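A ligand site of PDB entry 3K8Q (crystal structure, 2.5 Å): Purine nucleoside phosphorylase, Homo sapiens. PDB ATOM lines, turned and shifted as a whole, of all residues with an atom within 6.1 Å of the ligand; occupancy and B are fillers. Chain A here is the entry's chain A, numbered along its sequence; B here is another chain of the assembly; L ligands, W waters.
Water W1 lies within hydrogen-bond range of an oxygen (O3) of the ligand (2.7 Å) and the backbone NH (N) of Met 219 (3.2 Å).
The side-chain amide oxygen (OD1) of Asn 243 sits at hydrogen-bond distance from a nitrogen (N3) of the ligand (2.7 Å).
A nitrogen (N1) of the ligand is in hydrogen-bond range of the side-chain carboxylate (OE1) of Glu 201 (2.7 Å).
The side-chain hydroxyl of Tyr 88 is in hydrogen-bond range of an oxygen (O3) of the ligand, at 3.4 Å.
The backbone NH (N) of Gly 118 sits close to a nitrogen (N3) of the ligand (3.4 Å).
A ring nitrogen (ND1) of His 257 lies within hydrogen-bond range of an oxygen (O2) of the ligand, 3.4 Å away.
O of Val 217 sits close to N2 of the ligand (3.5 Å).
Ala 116 touches the ligand (O to C7, 3.1 Å).
Ala 117 touches the ligand.
Phe 200 touches the ligand (CE1 to C4, 3.6 Å).
Gly 218 touches the ligand.
Met 219 touches the ligand.
OG1 of Thr 242 touches N3 of the ligand (3.6 Å).
Val 245 touches the ligand (CG1 to O1, 3.6 Å).
Val 260 touches the ligand (CG1 to O2, 3.9 Å).
Phe 159 of chain B touches the ligand.
Hydrophobic or aromatic side chains within 4 Å of the ligand: Tyr 88, Phe 200, Val 217, Met 219, Val 245, His 257, Val 260 and Phe 159 of chain B.
The nearest printed residue that does not touch the ligand is His 86 (4.1 Å).
The backbone NH (N) of Gly 119 sits at hydrogen-bond distance from the backbone carbonyl oxygen (O) of Asn 243.
A ring nitrogen (ND1) of His 86 lies within hydrogen-bond range of the side-chain hydroxyl (OH) of Tyr 88 (3.1 Å).
O of Gly 118 is in hydrogen-bond range of N of Val 217 (3.0 Å).
OH of Tyr 192 is in hydrogen-bond range of N of Met 219 (3.1 Å).
The backbone carbonyl oxygen (O) of Gly 218 lies within hydrogen-bond range of the backbone NH (N) of Val 195 (3.0 Å).
N of Gly 218 lies close to OH of Tyr 192, 3.5 Å away.
The backbone carbonyl oxygen of Gly 119 lies within hydrogen-bond range of the backbone NH of Val 245 (3.1 Å).
The backbone NH (N) of Thr 242 is in hydrogen-bond range of the backbone carbonyl oxygen (O) of Ala 117.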
ATOM      1  N   SER A  33     -33.682  -2.498 -16.995  1.00  0.00           N
ATOM      2  CA  SER A  33     -33.559  -2.771 -18.434  1.00  0.00           C
ATOM      3  C   SER A  33     -33.370  -4.293 -18.748  1.00  0.00           C
ATOM      4  O   SER A  33     -34.079  -4.851 -19.630  1.00  0.00           O
ATOM      5  CB  SER A  33     -32.467  -1.913 -19.077  1.00  0.00           C
ATOM      6  OG  SER A  33     -31.204  -2.131 -18.463  1.00  0.00           O
ATOM      7  N   HIS A  86     -34.362   7.673 -15.487  1.00  0.00           N
ATOM      8  CA  HIS A  86     -33.020   7.973 -15.016  1.00  0.00           C
ATOM      9  C   HIS A  86     -32.731   9.480 -15.061  1.00  0.00           C
ATOM     10  O   HIS A  86     -33.277  10.206 -15.905  1.00  0.00           O
ATOM     11  CB  HIS A  86     -31.955   7.274 -15.871  1.00  0.00           C
ATOM     12  CG  HIS A  86     -32.256   5.832 -16.148  1.00  0.00           C
ATOM     13  ND1 HIS A  86     -33.084   5.443 -17.182  1.00  0.00           N
ATOM     14  CD2 HIS A  86     -31.833   4.695 -15.549  1.00  0.00           C
ATOM     15  CE1 HIS A  86     -33.167   4.116 -17.201  1.00  0.00           C
ATOM     16  NE2 HIS A  86     -32.409   3.646 -16.222  1.00  0.00           N
ATOM     17  N   TYR A  88     -29.976  10.796 -15.979  1.00  0.00           N
ATOM     18  CA  TYR A  88     -29.253  11.149 -17.201  1.00  0.00           C
ATOM     19  C   TYR A  88     -30.202  11.453 -18.381  1.00  0.00           C
ATOM     20  O   TYR A  88     -29.749  11.993 -19.381  1.00  0.00           O
ATOM     21  CB  TYR A  88     -28.228  10.062 -17.600  1.00  0.00           C
ATOM     22  CG  TYR A  88     -28.856   8.745 -17.988  1.00  0.00           C
ATOM     23  CD1 TYR A  88     -29.668   8.650 -19.127  1.00  0.00           C
ATOM     24  CD2 TYR A  88     -28.666   7.596 -17.210  1.00  0.00           C
ATOM     25  CE1 TYR A  88     -30.279   7.437 -19.488  1.00  0.00           C
ATOM     26  CE2 TYR A  88     -29.266   6.378 -17.547  1.00  0.00           C
ATOM     27  CZ  TYR A  88     -30.064   6.297 -18.690  1.00  0.00           C
ATOM     28  OH  TYR A  88     -30.663   5.102 -19.046  1.00  0.00           O
ATOM     29  N   ALA A 116     -29.327  -3.498 -14.340  1.00  0.00           N
ATOM     30  CA  ALA A 116     -28.076  -4.013 -14.893  1.00  0.00           C
ATOM     31  C   ALA A 116     -26.919  -3.167 -14.344  1.00  0.00           C
ATOM     32  O   ALA A 116     -27.119  -2.002 -14.040  1.00  0.00           O
ATOM     33  CB  ALA A 116     -28.107  -3.893 -16.405  1.00  0.00           C
ATOM     34  N   ALA A 117     -25.731  -3.730 -14.190  1.00  0.00           N
ATOM     35  CA  ALA A 117     -24.602  -2.961 -13.712  1.00  0.00           C
ATOM     36  C   ALA A 117     -23.310  -3.539 -14.201  1.00  0.00           C
ATOM     37  O   ALA A 117     -23.237  -4.715 -14.574  1.00  0.00           O
ATOM     38  CB  ALA A 117     -24.621  -2.872 -12.227  1.00  0.00           C
ATOM     39  N   GLY A 118     -22.291  -2.706 -14.190  1.00  0.00           N
ATOM     40  CA  GLY A 118     -20.966  -3.123 -14.587  1.00  0.00           C
ATOM     41  C   GLY A 118     -20.235  -3.603 -13.368  1.00  0.00           C
ATOM     42  O   GLY A 118     -20.416  -3.044 -12.271  1.00  0.00           O
ATOM     43  N   GLY A 119     -19.402  -4.625 -13.571  1.00  0.00           N
ATOM     44  CA  GLY A 119     -18.746  -5.305 -12.479  1.00  0.00           C
ATOM     45  C   GLY A 119     -17.482  -4.599 -12.075  1.00  0.00           C
ATOM     46  O   GLY A 119     -16.612  -4.382 -12.916  1.00  0.00           O
ATOM     47  N   TYR A 192     -23.584  -1.471  -4.340  1.00  0.00           N
ATOM     48  CA  TYR A 192     -23.889  -0.806  -5.613  1.00  0.00           C
ATOM     49  C   TYR A 192     -23.558   0.686  -5.515  1.00  0.00           C
ATOM     50  O   TYR A 192     -24.042   1.394  -4.621  1.00  0.00           O
ATOM     51  CB  TYR A 192     -25.371  -0.979  -5.949  1.00  0.00           C
ATOM     52  CG  TYR A 192     -25.874  -0.266  -7.162  1.00  0.00           C
ATOM     53  CD1 TYR A 192     -25.970  -0.921  -8.393  1.00  0.00           C
ATOM     54  CD2 TYR A 192     -26.304   1.069  -7.092  1.00  0.00           C
ATOM     55  CE1 TYR A 192     -26.475  -0.268  -9.528  1.00  0.00           C
ATOM     56  CE2 TYR A 192     -26.824   1.721  -8.229  1.00  0.00           C
ATOM     57  CZ  TYR A 192     -26.901   1.043  -9.425  1.00  0.00           C
ATOM     58  OH  TYR A 192     -27.385   1.656 -10.529  1.00  0.00           O
ATOM     59  N   VAL A 195     -23.786   6.286 -10.148  1.00  0.00           N
ATOM     60  CA  VAL A 195     -23.234   7.490 -10.826  1.00  0.00           C
ATOM     61  C   VAL A 195     -24.288   7.952 -11.834  1.00  0.00           C
ATOM     62  O   VAL A 195     -25.220   7.190 -12.165  1.00  0.00           O
ATOM     63  CB  VAL A 195     -21.894   7.248 -11.563  1.00  0.00           C
ATOM     64  CG1 VAL A 195     -20.781   6.819 -10.592  1.00  0.00           C
ATOM     65  CG2 VAL A 195     -22.062   6.285 -12.679  1.00  0.00           C
ATOM     66  N   PRO A 198     -24.685   9.993 -18.612  1.00  0.00           N
ATOM     67  CA  PRO A 198     -24.914   8.705 -19.268  1.00  0.00           C
ATOM     68  C   PRO A 198     -23.694   8.083 -19.967  1.00  0.00           C
ATOM     69  O   PRO A 198     -23.822   6.979 -20.519  1.00  0.00           O
ATOM     70  CB  PRO A 198     -25.967   9.044 -20.314  1.00  0.00           C
ATOM     71  CG  PRO A 198     -25.626  10.494 -20.709  1.00  0.00           C
ATOM     72  CD  PRO A 198     -25.012  11.133 -19.493  1.00  0.00           C
ATOM     73  N   SER A 199     -22.557   8.766 -19.998  1.00  0.00           N
ATOM     74  CA  SER A 199     -21.386   8.207 -20.633  1.00  0.00           C
ATOM     75  C   SER A 199     -20.765   7.189 -19.670  1.00  0.00           C
ATOM     76  O   SER A 199     -21.063   7.228 -18.467  1.00  0.00           O
ATOM     77  CB  SER A 199     -20.381   9.313 -21.018  1.00  0.00           C
ATOM     78  OG  SER A 199     -20.087  10.155 -19.910  1.00  0.00           O
ATOM     79  N   PHE A 200     -19.928   6.288 -20.193  1.00  0.00           N
ATOM     80  CA  PHE A 200     -19.366   5.222 -19.362  1.00  0.00           C
ATOM     81  C   PHE A 200     -18.065   5.679 -18.711  1.00  0.00           C
ATOM     82  O   PHE A 200     -17.405   6.633 -19.151  1.00  0.00           O
ATOM     83  CB  PHE A 200     -19.129   3.924 -20.141  1.00  0.00           C
ATOM     84  CG  PHE A 200     -20.394   3.116 -20.459  1.00  0.00           C
ATOM     85  CD1 PHE A 200     -21.164   2.572 -19.438  1.00  0.00           C
ATOM     86  CD2 PHE A 200     -20.739   2.834 -21.801  1.00  0.00           C
ATOM     87  CE1 PHE A 200     -22.300   1.779 -19.711  1.00  0.00           C
ATOM     88  CE2 PHE A 200     -21.871   2.043 -22.107  1.00  0.00           C
ATOM     89  CZ  PHE A 200     -22.668   1.509 -21.040  1.00  0.00           C
ATOM     90  N   GLU A 201     -17.712   4.996 -17.652  1.00  0.00           N
ATOM     91  CA  GLU A 201     -16.591   5.378 -16.812  1.00  0.00           C
ATOM     92  C   GLU A 201     -15.283   5.193 -17.555  1.00  0.00           C
ATOM     93  O   GLU A 201     -15.173   4.348 -18.449  1.00  0.00           O
ATOM     94  CB  GLU A 201     -16.551   4.496 -15.555  1.00  0.00           C
ATOM     95  CG  GLU A 201     -17.765   4.562 -14.663  1.00  0.00           C
ATOM     96  CD  GLU A 201     -19.044   3.990 -15.297  1.00  0.00           C
ATOM     97  OE1 GLU A 201     -19.017   2.874 -15.876  1.00  0.00           O
ATOM     98  OE2 GLU A 201     -20.086   4.678 -15.197  1.00  0.00           O
ATOM     99  N   VAL A 217     -21.496  -0.838 -10.483  1.00  0.00           N
ATOM    100  CA  VAL A 217     -21.840   0.543 -10.832  1.00  0.00           C
ATOM    101  C   VAL A 217     -22.998   0.619 -11.819  1.00  0.00           C
ATOM    102  O   VAL A 217     -22.975  -0.026 -12.851  1.00  0.00           O
ATOM    103  CB  VAL A 217     -20.610   1.266 -11.388  1.00  0.00           C
ATOM    104  CG1 VAL A 217     -20.046   0.506 -12.565  1.00  0.00           C
ATOM    105  CG2 VAL A 217     -20.975   2.709 -11.788  1.00  0.00           C
ATOM    106  N   GLY A 218     -24.031   1.387 -11.489  1.00  0.00           N
ATOM    107  CA  GLY A 218     -25.085   1.720 -12.457  1.00  0.00           C
ATOM    108  C   GLY A 218     -25.511   3.166 -12.322  1.00  0.00           C
ATOM    109  O   GLY A 218     -24.854   3.953 -11.606  1.00  0.00           O
ATOM    110  N   MET A 219     -26.647   3.510 -12.957  1.00  0.00           N
ATOM    111  CA  MET A 219     -27.106   4.885 -13.048  1.00  0.00           C
ATOM    112  C   MET A 219     -28.531   5.053 -12.577  1.00  0.00           C
ATOM    113  O   MET A 219     -29.210   6.031 -12.943  1.00  0.00           O
ATOM    114  CB  MET A 219     -26.931   5.407 -14.475  1.00  0.00           C
ATOM    115  CG  MET A 219     -25.491   5.163 -15.022  1.00  0.00           C
ATOM    116  SD  MET A 219     -25.279   5.643 -16.743  1.00  0.00           S
ATOM    117  CE  MET A 219     -23.545   5.228 -17.101  1.00  0.00           C
ATOM    118  N   LEU A 240     -27.864  -7.284 -12.262  1.00  0.00           N
ATOM    119  CA  LEU A 240     -27.300  -8.227 -13.179  1.00  0.00           C
ATOM    120  C   LEU A 240     -26.003  -7.658 -13.707  1.00  0.00           C
ATOM    121  O   LEU A 240     -25.968  -6.580 -14.269  1.00  0.00           O
ATOM    122  CB  LEU A 240     -28.296  -8.511 -14.313  1.00  0.00           C
ATOM    123  CG  LEU A 240     -27.776  -9.212 -15.585  1.00  0.00           C
ATOM    124  CD1 LEU A 240     -27.189 -10.587 -15.246  1.00  0.00           C
ATOM    125  CD2 LEU A 240     -28.870  -9.337 -16.677  1.00  0.00           C
ATOM    126  N   THR A 242     -23.654  -7.155 -16.338  1.00  0.00           N
ATOM    127  CA  THR A 242     -23.764  -7.315 -17.760  1.00  0.00           C
ATOM    128  C   THR A 242     -22.386  -7.191 -18.411  1.00  0.00           C
ATOM    129  O   THR A 242     -22.226  -7.510 -19.575  1.00  0.00           O
ATOM    130  CB  THR A 242     -24.624  -6.205 -18.327  1.00  0.00           C
ATOM    131  OG1 THR A 242     -24.167  -4.973 -17.756  1.00  0.00           O
ATOM    132  CG2 THR A 242     -26.071  -6.405 -17.949  1.00  0.00           C
ATOM    133  N   ASN A 243     -21.412  -6.722 -17.661  1.00  0.00           N
ATOM    134  CA  ASN A 243     -20.111  -6.405 -18.227  1.00  0.00           C
ATOM    135  C   ASN A 243     -19.139  -6.180 -17.084  1.00  0.00           C
ATOM    136  O   ASN A 243     -19.548  -5.868 -15.986  1.00  0.00           O
ATOM    137  CB  ASN A 243     -20.193  -5.167 -19.133  1.00  0.00           C
ATOM    138  CG  ASN A 243     -20.707  -3.901 -18.404  1.00  0.00           C
ATOM    139  OD1 ASN A 243     -21.892  -3.749 -18.087  1.00  0.00           O
ATOM    140  ND2 ASN A 243     -19.795  -2.983 -18.139  1.00  0.00           N
ATOM    141  N   VAL A 245     -16.149  -3.818 -15.907  1.00  0.00           N
ATOM    142  CA  VAL A 245     -15.720  -2.491 -16.348  1.00  0.00           C
ATOM    143  C   VAL A 245     -14.222  -2.548 -16.669  1.00  0.00           C
ATOM    144  O   VAL A 245     -13.458  -3.258 -15.995  1.00  0.00           O
ATOM    145  CB  VAL A 245     -16.088  -1.364 -15.357  1.00  0.00           C
ATOM    146  CG1 VAL A 245     -17.580  -1.406 -15.017  1.00  0.00           C
ATOM    147  CG2 VAL A 245     -15.276  -1.491 -14.106  1.00  0.00           C
ATOM    148  N   ALA A 255     -16.748  -0.640 -22.969  1.00  0.00           N
ATOM    149  CA  ALA A 255     -18.119  -0.785 -22.483  1.00  0.00           C
ATOM    150  C   ALA A 255     -19.097  -0.239 -23.536  1.00  0.00           C
ATOM    151  O   ALA A 255     -18.896   0.861 -24.061  1.00  0.00           O
ATOM    152  CB  ALA A 255     -18.305  -0.074 -21.143  1.00  0.00           C
ATOM    153  N   HIS A 257     -23.573  -0.444 -25.035  1.00  0.00           N
ATOM    154  CA  HIS A 257     -24.974  -0.751 -24.792  1.00  0.00           C
ATOM    155  C   HIS A 257     -25.474  -2.057 -25.427  1.00  0.00           C
ATOM    156  O   HIS A 257     -26.372  -2.717 -24.879  1.00  0.00           O
ATOM    157  CB  HIS A 257     -25.820   0.434 -25.289  1.00  0.00           C
ATOM    158  CG  HIS A 257     -27.280   0.338 -24.934  1.00  0.00           C
ATOM    159  ND1 HIS A 257     -27.723   0.058 -23.656  1.00  0.00           N
ATOM    160  CD2 HIS A 257     -28.386   0.555 -25.677  1.00  0.00           C
ATOM    161  CE1 HIS A 257     -29.042   0.077 -23.631  1.00  0.00           C
ATOM    162  NE2 HIS A 257     -29.471   0.370 -24.849  1.00  0.00           N
ATOM    163  N   VAL A 260     -24.538  -4.951 -23.233  1.00  0.00           N
ATOM    164  CA  VAL A 260     -25.356  -4.889 -21.997  1.00  0.00           C
ATOM    165  C   VAL A 260     -26.764  -5.447 -22.252  1.00  0.00           C
ATOM    166  O   VAL A 260     -27.272  -6.240 -21.451  1.00  0.00           O
ATOM    167  CB  VAL A 260     -25.421  -3.436 -21.397  1.00  0.00           C
ATOM    168  CG1 VAL A 260     -26.410  -3.358 -20.236  1.00  0.00           C
ATOM    169  CG2 VAL A 260     -24.047  -2.977 -20.953  1.00  0.00           C
ATOM    170  N   PHE B 159     -25.047   6.082 -24.630  1.00  0.00           N
ATOM    171  CA  PHE B 159     -24.067   5.719 -23.618  1.00  0.00           C
ATOM    172  C   PHE B 159     -22.682   5.550 -24.237  1.00  0.00           C
ATOM    173  O   PHE B 159     -22.194   4.441 -24.357  1.00  0.00           O
ATOM    174  CB  PHE B 159     -24.483   4.380 -22.963  1.00  0.00           C
ATOM    175  CG  PHE B 159     -25.894   4.333 -22.457  1.00  0.00           C
ATOM    176  CD1 PHE B 159     -26.274   4.995 -21.312  1.00  0.00           C
ATOM    177  CD2 PHE B 159     -26.859   3.571 -23.120  1.00  0.00           C
ATOM    178  CE1 PHE B 159     -27.619   4.953 -20.820  1.00  0.00           C
ATOM    179  CE2 PHE B 159     -28.215   3.494 -22.637  1.00  0.00           C
ATOM    180  CZ  PHE B 159     -28.571   4.192 -21.481  1.00  0.00           C
HETATM  181  N1  LIG L   1     -21.387   1.512 -15.982  1.00  0.00           N
HETATM  182  C1  LIG L   1     -22.489   2.190 -15.604  1.00  0.00           C
HETATM  183  N2  LIG L   1     -23.731   1.701 -15.743  1.00  0.00           N
HETATM  184  C2  LIG L   1     -23.890   0.474 -16.294  1.00  0.00           C
HETATM  185  C3  LIG L   1     -22.780  -0.343 -16.582  1.00  0.00           C
HETATM  186  C4  LIG L   1     -21.458   0.290 -16.565  1.00  0.00           C
HETATM  187  O1  LIG L   1     -20.425  -0.346 -16.872  1.00  0.00           O
HETATM  188  N3  LIG L   1     -23.234  -1.537 -17.266  1.00  0.00           N
HETATM  189  C5  LIG L   1     -24.602  -1.464 -17.107  1.00  0.00           C
HETATM  190  C6  LIG L   1     -25.044  -0.273 -16.511  1.00  0.00           C
HETATM  191  N4  LIG L   1     -27.027   0.506 -17.569  1.00  0.00           N
HETATM  192  C7  LIG L   1     -26.476   0.119 -16.274  1.00  0.00           C
HETATM  193  C8  LIG L   1     -26.568   1.752 -18.212  1.00  0.00           C
HETATM  194  C9  LIG L   1     -27.506   2.896 -17.868  1.00  0.00           C
HETATM  195  C10 LIG L   1     -26.393   1.646 -19.733  1.00  0.00           C
HETATM  196  O2  LIG L   1     -27.018   0.483 -20.325  1.00  0.00           O
HETATM  197  O3  LIG L   1     -28.898   2.495 -17.891  1.00  0.00           O
HETATM  198  O   HOH W   1     -28.630   2.595 -15.234  1.00  0.00           O
